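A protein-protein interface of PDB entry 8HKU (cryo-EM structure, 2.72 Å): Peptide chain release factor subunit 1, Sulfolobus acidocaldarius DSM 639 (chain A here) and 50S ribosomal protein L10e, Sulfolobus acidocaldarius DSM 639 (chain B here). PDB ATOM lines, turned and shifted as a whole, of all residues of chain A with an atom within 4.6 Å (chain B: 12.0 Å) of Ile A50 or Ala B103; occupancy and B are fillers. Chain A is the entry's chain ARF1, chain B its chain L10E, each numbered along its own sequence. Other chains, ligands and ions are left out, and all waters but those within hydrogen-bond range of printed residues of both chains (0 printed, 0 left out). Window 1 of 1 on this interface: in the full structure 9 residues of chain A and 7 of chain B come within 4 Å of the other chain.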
ATOM      1  N   MET A  39     -19.197 -14.241  10.335  1.00  0.00           N
ATOM      2  CA  MET A  39     -18.650 -14.166  11.678  1.00  0.00           C
ATOM      3  C   MET A  39     -18.932 -12.791  12.286  1.00  0.00           C
ATOM      4  O   MET A  39     -19.076 -11.791  11.579  1.00  0.00           O
ATOM      5  CB  MET A  39     -17.149 -14.454  11.638  1.00  0.00           C
ATOM      6  CG  MET A  39     -16.829 -15.868  11.200  1.00  0.00           C
ATOM      7  SD  MET A  39     -17.456 -17.093  12.356  1.00  0.00           S
ATOM      8  CE  MET A  39     -17.132 -18.592  11.441  1.00  0.00           C
ATOM      9  N   ARG A  46      -9.081 -16.411  16.237  1.00  0.00           N
ATOM     10  CA  ARG A  46     -10.059 -17.441  16.530  1.00  0.00           C
ATOM     11  C   ARG A  46     -11.162 -17.568  15.494  1.00  0.00           C
ATOM     12  O   ARG A  46     -11.889 -18.560  15.524  1.00  0.00           O
ATOM     13  CB  ARG A  46     -10.683 -17.207  17.907  1.00  0.00           C
ATOM     14  CG  ARG A  46     -11.460 -15.943  18.034  1.00  0.00           C
ATOM     15  CD  ARG A  46     -12.071 -15.876  19.406  1.00  0.00           C
ATOM     16  NE  ARG A  46     -11.063 -15.823  20.458  1.00  0.00           N
ATOM     17  CZ  ARG A  46     -10.863 -16.776  21.358  1.00  0.00           C
ATOM     18  NH1 ARG A  46     -11.595 -17.876  21.373  1.00  0.00           N
ATOM     19  NH2 ARG A  46      -9.908 -16.617  22.271  1.00  0.00           N
ATOM     20  N   ILE A  47     -11.313 -16.606  14.585  1.00  0.00           N
ATOM     21  CA  ILE A  47     -12.185 -16.834  13.436  1.00  0.00           C
ATOM     22  C   ILE A  47     -11.638 -17.967  12.580  1.00  0.00           C
ATOM     23  O   ILE A  47     -12.390 -18.825  12.105  1.00  0.00           O
ATOM     24  CB  ILE A  47     -12.362 -15.543  12.619  1.00  0.00           C
ATOM     25  CG1 ILE A  47     -13.291 -14.572  13.343  1.00  0.00           C
ATOM     26  CG2 ILE A  47     -12.904 -15.853  11.237  1.00  0.00           C
ATOM     27  CD1 ILE A  47     -13.291 -13.190  12.746  1.00  0.00           C
ATOM     28  N   GLU A  48     -10.319 -17.995  12.378  1.00  0.00           N
ATOM     29  CA  GLU A  48      -9.699 -19.056  11.596  1.00  0.00           C
ATOM     30  C   GLU A  48      -9.827 -20.420  12.255  1.00  0.00           C
ATOM     31  O   GLU A  48      -9.644 -21.437  11.579  1.00  0.00           O
ATOM     32  CB  GLU A  48      -8.226 -18.734  11.353  1.00  0.00           C
ATOM     33  CG  GLU A  48      -7.999 -17.529  10.461  1.00  0.00           C
ATOM     34  CD  GLU A  48      -6.532 -17.245  10.229  1.00  0.00           C
ATOM     35  OE1 GLU A  48      -5.693 -17.935  10.844  1.00  0.00           O
ATOM     36  OE2 GLU A  48      -6.217 -16.332   9.437  1.00  0.00           O
ATOM     37  N   ARG A  49     -10.118 -20.469  13.556  1.00  0.00           N
ATOM     38  CA  ARG A  49     -10.372 -21.750  14.205  1.00  0.00           C
ATOM     39  C   ARG A  49     -11.628 -22.408  13.655  1.00  0.00           C
ATOM     40  O   ARG A  49     -11.597 -23.575  13.250  1.00  0.00           O
ATOM     41  CB  ARG A  49     -10.493 -21.568  15.714  1.00  0.00           C
ATOM     42  CG  ARG A  49      -9.190 -21.314  16.428  1.00  0.00           C
ATOM     43  CD  ARG A  49      -9.389 -21.435  17.924  1.00  0.00           C
ATOM     44  NE  ARG A  49      -8.861 -20.269  18.615  1.00  0.00           N
ATOM     45  CZ  ARG A  49      -9.345 -19.782  19.748  1.00  0.00           C
ATOM     46  NH1 ARG A  49     -10.381 -20.338  20.353  1.00  0.00           N
ATOM     47  NH2 ARG A  49      -8.775 -18.709  20.285  1.00  0.00           N
ATOM     48  N   ILE A  50     -12.744 -21.676  13.623  1.00  0.00           N
ATOM     49  CA  ILE A  50     -14.000 -22.270  13.173  1.00  0.00           C
ATOM     50  C   ILE A  50     -13.892 -22.722  11.727  1.00  0.00           C
ATOM     51  O   ILE A  50     -14.303 -23.833  11.375  1.00  0.00           O
ATOM     52  CB  ILE A  50     -15.177 -21.292  13.336  1.00  0.00           C
ATOM     53  CG1 ILE A  50     -15.420 -20.921  14.789  1.00  0.00           C
ATOM     54  CG2 ILE A  50     -16.423 -21.886  12.768  1.00  0.00           C
ATOM     55  CD1 ILE A  50     -14.648 -19.756  15.205  1.00  0.00           C
ATOM     56  N   ILE A  51     -13.346 -21.865  10.865  1.00  0.00           N
ATOM     57  CA  ILE A  51     -13.270 -22.188   9.446  1.00  0.00           C
ATOM     58  C   ILE A  51     -12.408 -23.418   9.222  1.00  0.00           C
ATOM     59  O   ILE A  51     -12.607 -24.157   8.252  1.00  0.00           O
ATOM     60  CB  ILE A  51     -12.753 -20.967   8.664  1.00  0.00           C
ATOM     61  CG1 ILE A  51     -13.612 -19.749   8.989  1.00  0.00           C
ATOM     62  CG2 ILE A  51     -12.768 -21.234   7.170  1.00  0.00           C
ATOM     63  CD1 ILE A  51     -12.979 -18.450   8.606  1.00  0.00           C
ATOM     64  N   GLU A  52     -11.449 -23.666  10.108  1.00  0.00           N
ATOM     65  CA  GLU A  52     -10.615 -24.852  10.025  1.00  0.00           C
ATOM     66  C   GLU A  52     -11.086 -25.970  10.943  1.00  0.00           C
ATOM     67  O   GLU A  52     -10.411 -26.998  11.036  1.00  0.00           O
ATOM     68  CB  GLU A  52      -9.162 -24.500  10.339  1.00  0.00           C
ATOM     69  CG  GLU A  52      -8.458 -23.749   9.225  1.00  0.00           C
ATOM     70  CD  GLU A  52      -7.057 -23.329   9.609  1.00  0.00           C
ATOM     71  OE1 GLU A  52      -6.663 -23.583  10.767  1.00  0.00           O
ATOM     72  OE2 GLU A  52      -6.349 -22.751   8.758  1.00  0.00           O
ATOM     73  N   GLU A  53     -12.222 -25.804  11.618  1.00  0.00           N
ATOM     74  CA  GLU A  53     -12.692 -26.819  12.548  1.00  0.00           C
ATOM     75  C   GLU A  53     -13.991 -27.473  12.097  1.00  0.00           C
ATOM     76  O   GLU A  53     -14.077 -28.703  12.084  1.00  0.00           O
ATOM     77  CB  GLU A  53     -12.844 -26.241  13.952  1.00  0.00           C
ATOM     78  CG  GLU A  53     -13.302 -27.270  14.939  1.00  0.00           C
ATOM     79  CD  GLU A  53     -13.044 -26.851  16.358  1.00  0.00           C
ATOM     80  OE1 GLU A  53     -12.480 -25.755  16.570  1.00  0.00           O
ATOM     81  OE2 GLU A  53     -13.365 -27.645  17.258  1.00  0.00           O
ATOM     82  N   MET A  54     -15.019 -26.706  11.737  1.00  0.00           N
ATOM     83  CA  MET A  54     -16.131 -27.402  11.106  1.00  0.00           C
ATOM     84  C   MET A  54     -15.837 -27.757   9.657  1.00  0.00           C
ATOM     85  O   MET A  54     -16.637 -28.462   9.037  1.00  0.00           O
ATOM     86  CB  MET A  54     -17.448 -26.629  11.227  1.00  0.00           C
ATOM     87  CG  MET A  54     -17.563 -25.763  12.470  1.00  0.00           C
ATOM     88  SD  MET A  54     -19.200 -25.021  12.662  1.00  0.00           S
ATOM     89  CE  MET A  54     -19.112 -23.567  11.658  1.00  0.00           C
ATOM     90  N   TYR A  55     -14.716 -27.293   9.105  1.00  0.00           N
ATOM     91  CA  TYR A  55     -14.173 -27.952   7.925  1.00  0.00           C
ATOM     92  C   TYR A  55     -13.797 -29.390   8.246  1.00  0.00           C
ATOM     93  O   TYR A  55     -14.106 -30.310   7.482  1.00  0.00           O
ATOM     94  CB  TYR A  55     -12.961 -27.188   7.403  1.00  0.00           C
ATOM     95  CG  TYR A  55     -12.246 -27.869   6.260  1.00  0.00           C
ATOM     96  CD1 TYR A  55     -12.938 -28.295   5.136  1.00  0.00           C
ATOM     97  CD2 TYR A  55     -10.879 -28.081   6.304  1.00  0.00           C
ATOM     98  CE1 TYR A  55     -12.286 -28.914   4.090  1.00  0.00           C
ATOM     99  CE2 TYR A  55     -10.221 -28.700   5.265  1.00  0.00           C
ATOM    100  CZ  TYR A  55     -10.929 -29.115   4.162  1.00  0.00           C
ATOM    101  OH  TYR A  55     -10.272 -29.728   3.125  1.00  0.00           O
ATOM    102  N   ASN B  95     -17.958 -30.252  27.726  1.00  0.00           N
ATOM    103  CA  ASN B  95     -17.945 -28.823  27.418  1.00  0.00           C
ATOM    104  C   ASN B  95     -17.447 -28.635  25.983  1.00  0.00           C
ATOM    105  O   ASN B  95     -16.354 -28.137  25.717  1.00  0.00           O
ATOM    106  CB  ASN B  95     -17.078 -28.084  28.421  1.00  0.00           C
ATOM    107  CG  ASN B  95     -17.299 -26.603  28.403  1.00  0.00           C
ATOM    108  OD1 ASN B  95     -18.206 -26.113  27.746  1.00  0.00           O
ATOM    109  ND2 ASN B  95     -16.464 -25.871  29.126  1.00  0.00           N
ATOM    110  N   LYS B  96     -18.305 -29.034  25.038  1.00  0.00           N
ATOM    111  CA  LYS B  96     -17.946 -29.038  23.625  1.00  0.00           C
ATOM    112  C   LYS B  96     -17.654 -27.649  23.114  1.00  0.00           C
ATOM    113  O   LYS B  96     -17.017 -27.507  22.070  1.00  0.00           O
ATOM    114  CB  LYS B  96     -19.079 -29.622  22.778  1.00  0.00           C
ATOM    115  CG  LYS B  96     -19.342 -31.089  22.998  1.00  0.00           C
ATOM    116  CD  LYS B  96     -20.509 -31.579  22.180  1.00  0.00           C
ATOM    117  CE  LYS B  96     -20.134 -31.636  20.717  1.00  0.00           C
ATOM    118  NZ  LYS B  96     -19.116 -32.692  20.479  1.00  0.00           N
ATOM    119  N   MET B  97     -18.111 -26.623  23.825  1.00  0.00           N
ATOM    120  CA  MET B  97     -18.013 -25.261  23.330  1.00  0.00           C
ATOM    121  C   MET B  97     -16.574 -24.851  23.065  1.00  0.00           C
ATOM    122  O   MET B  97     -16.343 -23.950  22.252  1.00  0.00           O
ATOM    123  CB  MET B  97     -18.697 -24.325  24.322  1.00  0.00           C
ATOM    124  CG  MET B  97     -17.814 -23.867  25.442  1.00  0.00           C
ATOM    125  SD  MET B  97     -18.715 -22.907  26.656  1.00  0.00           S
ATOM    126  CE  MET B  97     -17.436 -22.724  27.879  1.00  0.00           C
ATOM    127  N   MET B  98     -15.601 -25.525  23.687  1.00  0.00           N
ATOM    128  CA  MET B  98     -14.206 -25.338  23.303  1.00  0.00           C
ATOM    129  C   MET B  98     -13.987 -25.647  21.833  1.00  0.00           C
ATOM    130  O   MET B  98     -13.023 -25.164  21.232  1.00  0.00           O
ATOM    131  CB  MET B  98     -13.295 -26.223  24.144  1.00  0.00           C
ATOM    132  CG  MET B  98     -13.251 -25.897  25.617  1.00  0.00           C
ATOM    133  SD  MET B  98     -12.581 -24.275  25.964  1.00  0.00           S
ATOM    134  CE  MET B  98     -12.900 -24.180  27.715  1.00  0.00           C
ATOM    135  N   ALA B  99     -14.848 -26.470  21.242  1.00  0.00           N
ATOM    136  CA  ALA B  99     -14.753 -26.739  19.816  1.00  0.00           C
ATOM    137  C   ALA B  99     -15.342 -25.597  18.996  1.00  0.00           C
ATOM    138  O   ALA B  99     -14.616 -24.917  18.265  1.00  0.00           O
ATOM    139  CB  ALA B  99     -15.452 -28.056  19.474  1.00  0.00           C
ATOM    140  N   PHE B 100     -16.649 -25.362  19.121  1.00  0.00           N
ATOM    141  CA  PHE B 100     -17.317 -24.364  18.288  1.00  0.00           C
ATOM    142  C   PHE B 100     -17.454 -23.013  18.991  1.00  0.00           C
ATOM    143  O   PHE B 100     -16.943 -21.999  18.505  1.00  0.00           O
ATOM    144  CB  PHE B 100     -18.699 -24.873  17.857  1.00  0.00           C
ATOM    145  CG  PHE B 100     -19.544 -23.825  17.184  1.00  0.00           C
ATOM    146  CD1 PHE B 100     -19.148 -23.270  15.977  1.00  0.00           C
ATOM    147  CD2 PHE B 100     -20.717 -23.374  17.767  1.00  0.00           C
ATOM    148  CE1 PHE B 100     -19.916 -22.300  15.356  1.00  0.00           C
ATOM    149  CE2 PHE B 100     -21.487 -22.402  17.151  1.00  0.00           C
ATOM    150  CZ  PHE B 100     -21.085 -21.865  15.944  1.00  0.00           C
ATOM    151  N   ALA B 101     -18.140 -22.986  20.134  1.00  0.00           N
ATOM    152  CA  ALA B 101     -18.455 -21.720  20.785  1.00  0.00           C
ATOM    153  C   ALA B 101     -17.272 -21.125  21.532  1.00  0.00           C
ATOM    154  O   ALA B 101     -17.398 -20.022  22.073  1.00  0.00           O
ATOM    155  CB  ALA B 101     -19.631 -21.894  21.747  1.00  0.00           C
ATOM    156  N   GLY B 102     -16.148 -21.822  21.597  1.00  0.00           N
ATOM    157  CA  GLY B 102     -14.959 -21.290  22.220  1.00  0.00           C
ATOM    158  C   GLY B 102     -14.068 -20.490  21.302  1.00  0.00           C
ATOM    159  O   GLY B 102     -12.944 -20.151  21.689  1.00  0.00           O
ATOM    160  N   ALA B 103     -14.526 -20.185  20.086  1.00  0.00           N
ATOM    161  CA  ALA B 103     -13.669 -19.501  19.127  1.00  0.00           C
ATOM    162  C   ALA B 103     -14.410 -18.424  18.342  1.00  0.00           C
ATOM    163  O   ALA B 103     -13.828 -17.828  17.428  1.00  0.00           O
ATOM    164  CB  ALA B 103     -13.033 -20.512  18.170  1.00  0.00           C
ATOM    165  N   ASP B 104     -15.667 -18.141  18.678  1.00  0.00           N
ATOM    166  CA  ASP B 104     -16.411 -17.041  18.074  1.00  0.00           C
ATOM    167  C   ASP B 104     -16.318 -15.791  18.936  1.00  0.00           C
ATOM    168  O   ASP B 104     -17.116 -14.863  18.783  1.00  0.00           O
ATOM    169  CB  ASP B 104     -17.879 -17.418  17.866  1.00  0.00           C
ATOM    170  CG  ASP B 104     -18.082 -18.388  16.728  1.00  0.00           C
ATOM    171  OD1 ASP B 104     -17.305 -18.333  15.757  1.00  0.00           O
ATOM    172  OD2 ASP B 104     -19.023 -19.204  16.803  1.00  0.00           O
ATOM    173  N   ARG B 105     -15.366 -15.770  19.873  1.00  0.00           N
ATOM    174  CA  ARG B 105     -15.453 -14.893  21.039  1.00  0.00           C
ATOM    175  C   ARG B 105     -16.835 -15.010  21.675  1.00  0.00           C
ATOM    176  O   ARG B 105     -17.308 -14.102  22.360  1.00  0.00           O
ATOM    177  CB  ARG B 105     -15.123 -13.440  20.693  1.00  0.00           C
ATOM    178  CG  ARG B 105     -13.643 -13.126  20.559  1.00  0.00           C
ATOM    179  CD  ARG B 105     -12.888 -13.441  21.842  1.00  0.00           C
ATOM    180  NE  ARG B 105     -11.456 -13.204  21.696  1.00  0.00           N
ATOM    181  CZ  ARG B 105     -10.548 -13.463  22.628  1.00  0.00           C
ATOM    182  NH1 ARG B 105     -10.887 -13.972  23.800  1.00  0.00           N
ATOM    183  NH2 ARG B 105      -9.270 -13.201  22.379  1.00  0.00           N
ATOM    184  N   LEU B 106     -17.471 -16.159  21.445  1.00  0.00           N
ATOM    185  CA  LEU B 106     -18.738 -16.549  22.033  1.00  0.00           C
ATOM    186  C   LEU B 106     -18.377 -16.992  23.441  1.00  0.00           C
ATOM    187  O   LEU B 106     -17.282 -16.669  23.910  1.00  0.00           O
ATOM    188  CB  LEU B 106     -19.405 -17.646  21.196  1.00  0.00           C
ATOM    189  CG  LEU B 106     -20.929 -17.800  21.250  1.00  0.00           C
ATOM    190  CD1 LEU B 106     -21.626 -16.517  20.813  1.00  0.00           C
ATOM    191  CD2 LEU B 106     -21.398 -18.966  20.396  1.00  0.00           C
ATOM    192  N   GLN B 107     -19.235 -17.720  24.144  1.00  0.00           N
ATOM    193  CA  GLN B 107     -18.884 -17.969  25.537  1.00  0.00           C
ATOM    194  C   GLN B 107     -17.652 -18.874  25.627  1.00  0.00           C
ATOM    195  O   GLN B 107     -17.706 -20.012  26.102  1.00  0.00           O
ATOM    196  CB  GLN B 107     -20.095 -18.526  26.303  1.00  0.00           C
ATOM    197  CG  GLN B 107     -20.598 -19.923  25.919  1.00  0.00           C
ATOM    198  CD  GLN B 107     -21.592 -19.892  24.778  1.00  0.00           C
ATOM    199  OE1 GLN B 107     -21.711 -18.895  24.072  1.00  0.00           O
ATOM    200  NE2 GLN B 107     -22.318 -20.986  24.598  1.00  0.00           N
ATOM    201  N   ASP B 108     -16.515 -18.322  25.204  1.00  0.00           N
ATOM    202  CA  ASP B 108     -15.237 -19.005  25.121  1.00  0.00           C
ATOM    203  C   ASP B 108     -14.517 -18.974  26.462  1.00  0.00           C
ATOM    204  O   ASP B 108     -14.825 -18.177  27.347  1.00  0.00           O
ATOM    205  CB  ASP B 108     -14.368 -18.370  24.041  1.00  0.00           C
ATOM    206  CG  ASP B 108     -13.765 -17.059  24.475  1.00  0.00           C
ATOM    207  OD1 ASP B 108     -14.428 -16.315  25.224  1.00  0.00           O
ATOM    208  OD2 ASP B 108     -12.633 -16.758  24.050  1.00  0.00           O
ATOM    209  N   GLY B 109     -13.516 -19.839  26.589  1.00  0.00           N
ATOM    210  CA  GLY B 109     -12.909 -20.026  27.883  1.00  0.00           C
ATOM    211  C   GLY B 109     -13.815 -20.859  28.763  1.00  0.00           C
ATOM    212  O   GLY B 109     -14.585 -21.689  28.294  1.00  0.00           O
ATOM    213  N   MET B 110     -13.731 -20.626  30.062  1.00  0.00           N
ATOM    214  CA  MET B 110     -14.574 -21.329  31.010  1.00  0.00           C
ATOM    215  C   MET B 110     -15.885 -20.602  31.289  1.00  0.00           C
ATOM    216  O   MET B 110     -16.594 -20.980  32.220  1.00  0.00           O
ATOM    217  CB  MET B 110     -13.808 -21.570  32.308  1.00  0.00           C
ATOM    218  CG  MET B 110     -12.762 -22.675  32.226  1.00  0.00           C
ATOM    219  SD  MET B 110     -13.483 -24.304  32.063  1.00  0.00           S
ATOM    220  CE  MET B 110     -14.272 -24.491  33.646  1.00  0.00           C
ATOM    221  N   ARG B 111     -16.216 -19.570  30.518  1.00  0.00           N
ATOM    222  CA  ARG B 111     -17.484 -18.868  30.675  1.00  0.00           C
ATOM    223  C   ARG B 111     -18.637 -19.728  30.184  1.00  0.00           C
ATOM    224  O   ARG B 111     -18.626 -20.192  29.043  1.00  0.00           O
ATOM    225  CB  ARG B 111     -17.461 -17.557  29.895  1.00  0.00           C
ATOM    226  CG  ARG B 111     -18.837 -17.069  29.474  1.00  0.00           C
ATOM    227  CD  ARG B 111     -18.782 -15.779  28.711  1.00  0.00           C
ATOM    228  NE  ARG B 111     -18.336 -14.670  29.538  1.00  0.00           N
ATOM    229  CZ  ARG B 111     -18.333 -13.406  29.146  1.00  0.00           C
ATOM    230  NH1 ARG B 111     -18.769 -13.055  27.953  1.00  0.00           N
ATOM    231  NH2 ARG B 111     -17.864 -12.475  29.965  1.00  0.00           N
ATOM    232  N   LEU B 112     -19.656 -19.897  31.029  1.00  0.00           N
ATOM    233  CA  LEU B 112     -20.804 -20.757  30.747  1.00  0.00           C
ATOM    234  C   LEU B 112     -20.350 -22.179  30.426  1.00  0.00           C
ATOM    235  O   LEU B 112     -20.562 -22.698  29.334  1.00  0.00           O
ATOM    236  CB  LEU B 112     -21.665 -20.185  29.617  1.00  0.00           C
ATOM    237  CG  LEU B 112     -22.463 -18.915  29.902  1.00  0.00           C
ATOM    238  CD1 LEU B 112     -23.000 -18.353  28.622  1.00  0.00           C
ATOM    239  CD2 LEU B 112     -23.584 -19.193  30.872  1.00  0.00           C
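O of Gly B102 lies within hydrogen-bond range of NH1 of Arg A46 (2.7 Å).
The guanidinium group (NH1) of Arg A49 is in hydrogen-bond range of the backbone carbonyl oxygen (O) of Gly B102, 2.9 Å away.
The guanidinium group (NH1) of Arg A46 lies within salt-bridge range of the side-chain carboxylate (OD2) of Asp B108 (3.1 Å).
The side-chain sulfur of Met A39 sits close to the side-chain carboxylate of Asp B104 (3.6 Å).
The backbone carbonyl oxygen of Arg A46 lies close to the backbone carbonyl oxygen of Ala B103, at 2.8 Å.
The guanidinium group of Arg A46 lies close to the guanidinium group of Arg B105.
O of Ala B99 lies close to OE1 of Glu A53, at 2.9 Å.
NH1 of Arg B105 lies within salt-bridge range of OD2 of Asp B108 (3.3 Å).
Ala B103 touches Ile A47.
NH1 of Arg A49 touches CB of Ala B103, 3.4 Å away.
Ala B103 touches Ile A50 (O to CD1, 3.1 Å).
OD1 of Asp B104 touches CD1 of Ile A50, 3.1 Å away.
Phe B100 touches Met A54.
Of chain B, only Gly B102 (2.7 Å), Ala B103 (2.8 Å), Arg B105 (2.9 Å) and Asp B108 (3.1 Å) come within 4 Å of Arg A46.
Printed residues of chain B within 4 Å of Ile A47: Ala B103 (3.99 Å).
Arg A49 touches just these residues of chain B: Gly B102 (2.9 Å) and Ala B103 (3.4 Å).
Of chain B, only Ala B103 and Asp B104 come within 4 Å of Ile A50.
No residue of chain B comes within 4 Å of Ile A51.
Glu A53 touches just one residue of chain B: Ala B99 (2.9 Å).
Met A54 touches just one residue of chain B: Phe B100 (3.7 Å).
Of the printed residues of chain A, Ala B99 touches Glu A53 (2.9 Å).
Printed residues of chain A within 4 Å of Ala B103: Arg A46, Ile A47, Arg A49 and Ile A50.
Of the printed residues of chain A, Asp B104 touches Met A39 (3.6 Å) and Ile A50 (3.1 Å).
Printed residues of chain A within 4 Å of Asp B108: Arg A46 (3.1 Å).
Printed residues of chain A that touch a printed residue of chain B: Met A39, Arg A46, Ile A47, Arg A49, Ile A50, Glu A53 and Met A54.
Among the printed residues, 12 pairs touch across the chains.
Among the printed residues, Asp or Glu carboxylates within 4 Å of a Lys or Arg side-chain nitrogen of the other chain: Arg A46 with Asp B108 (3.1 Å).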
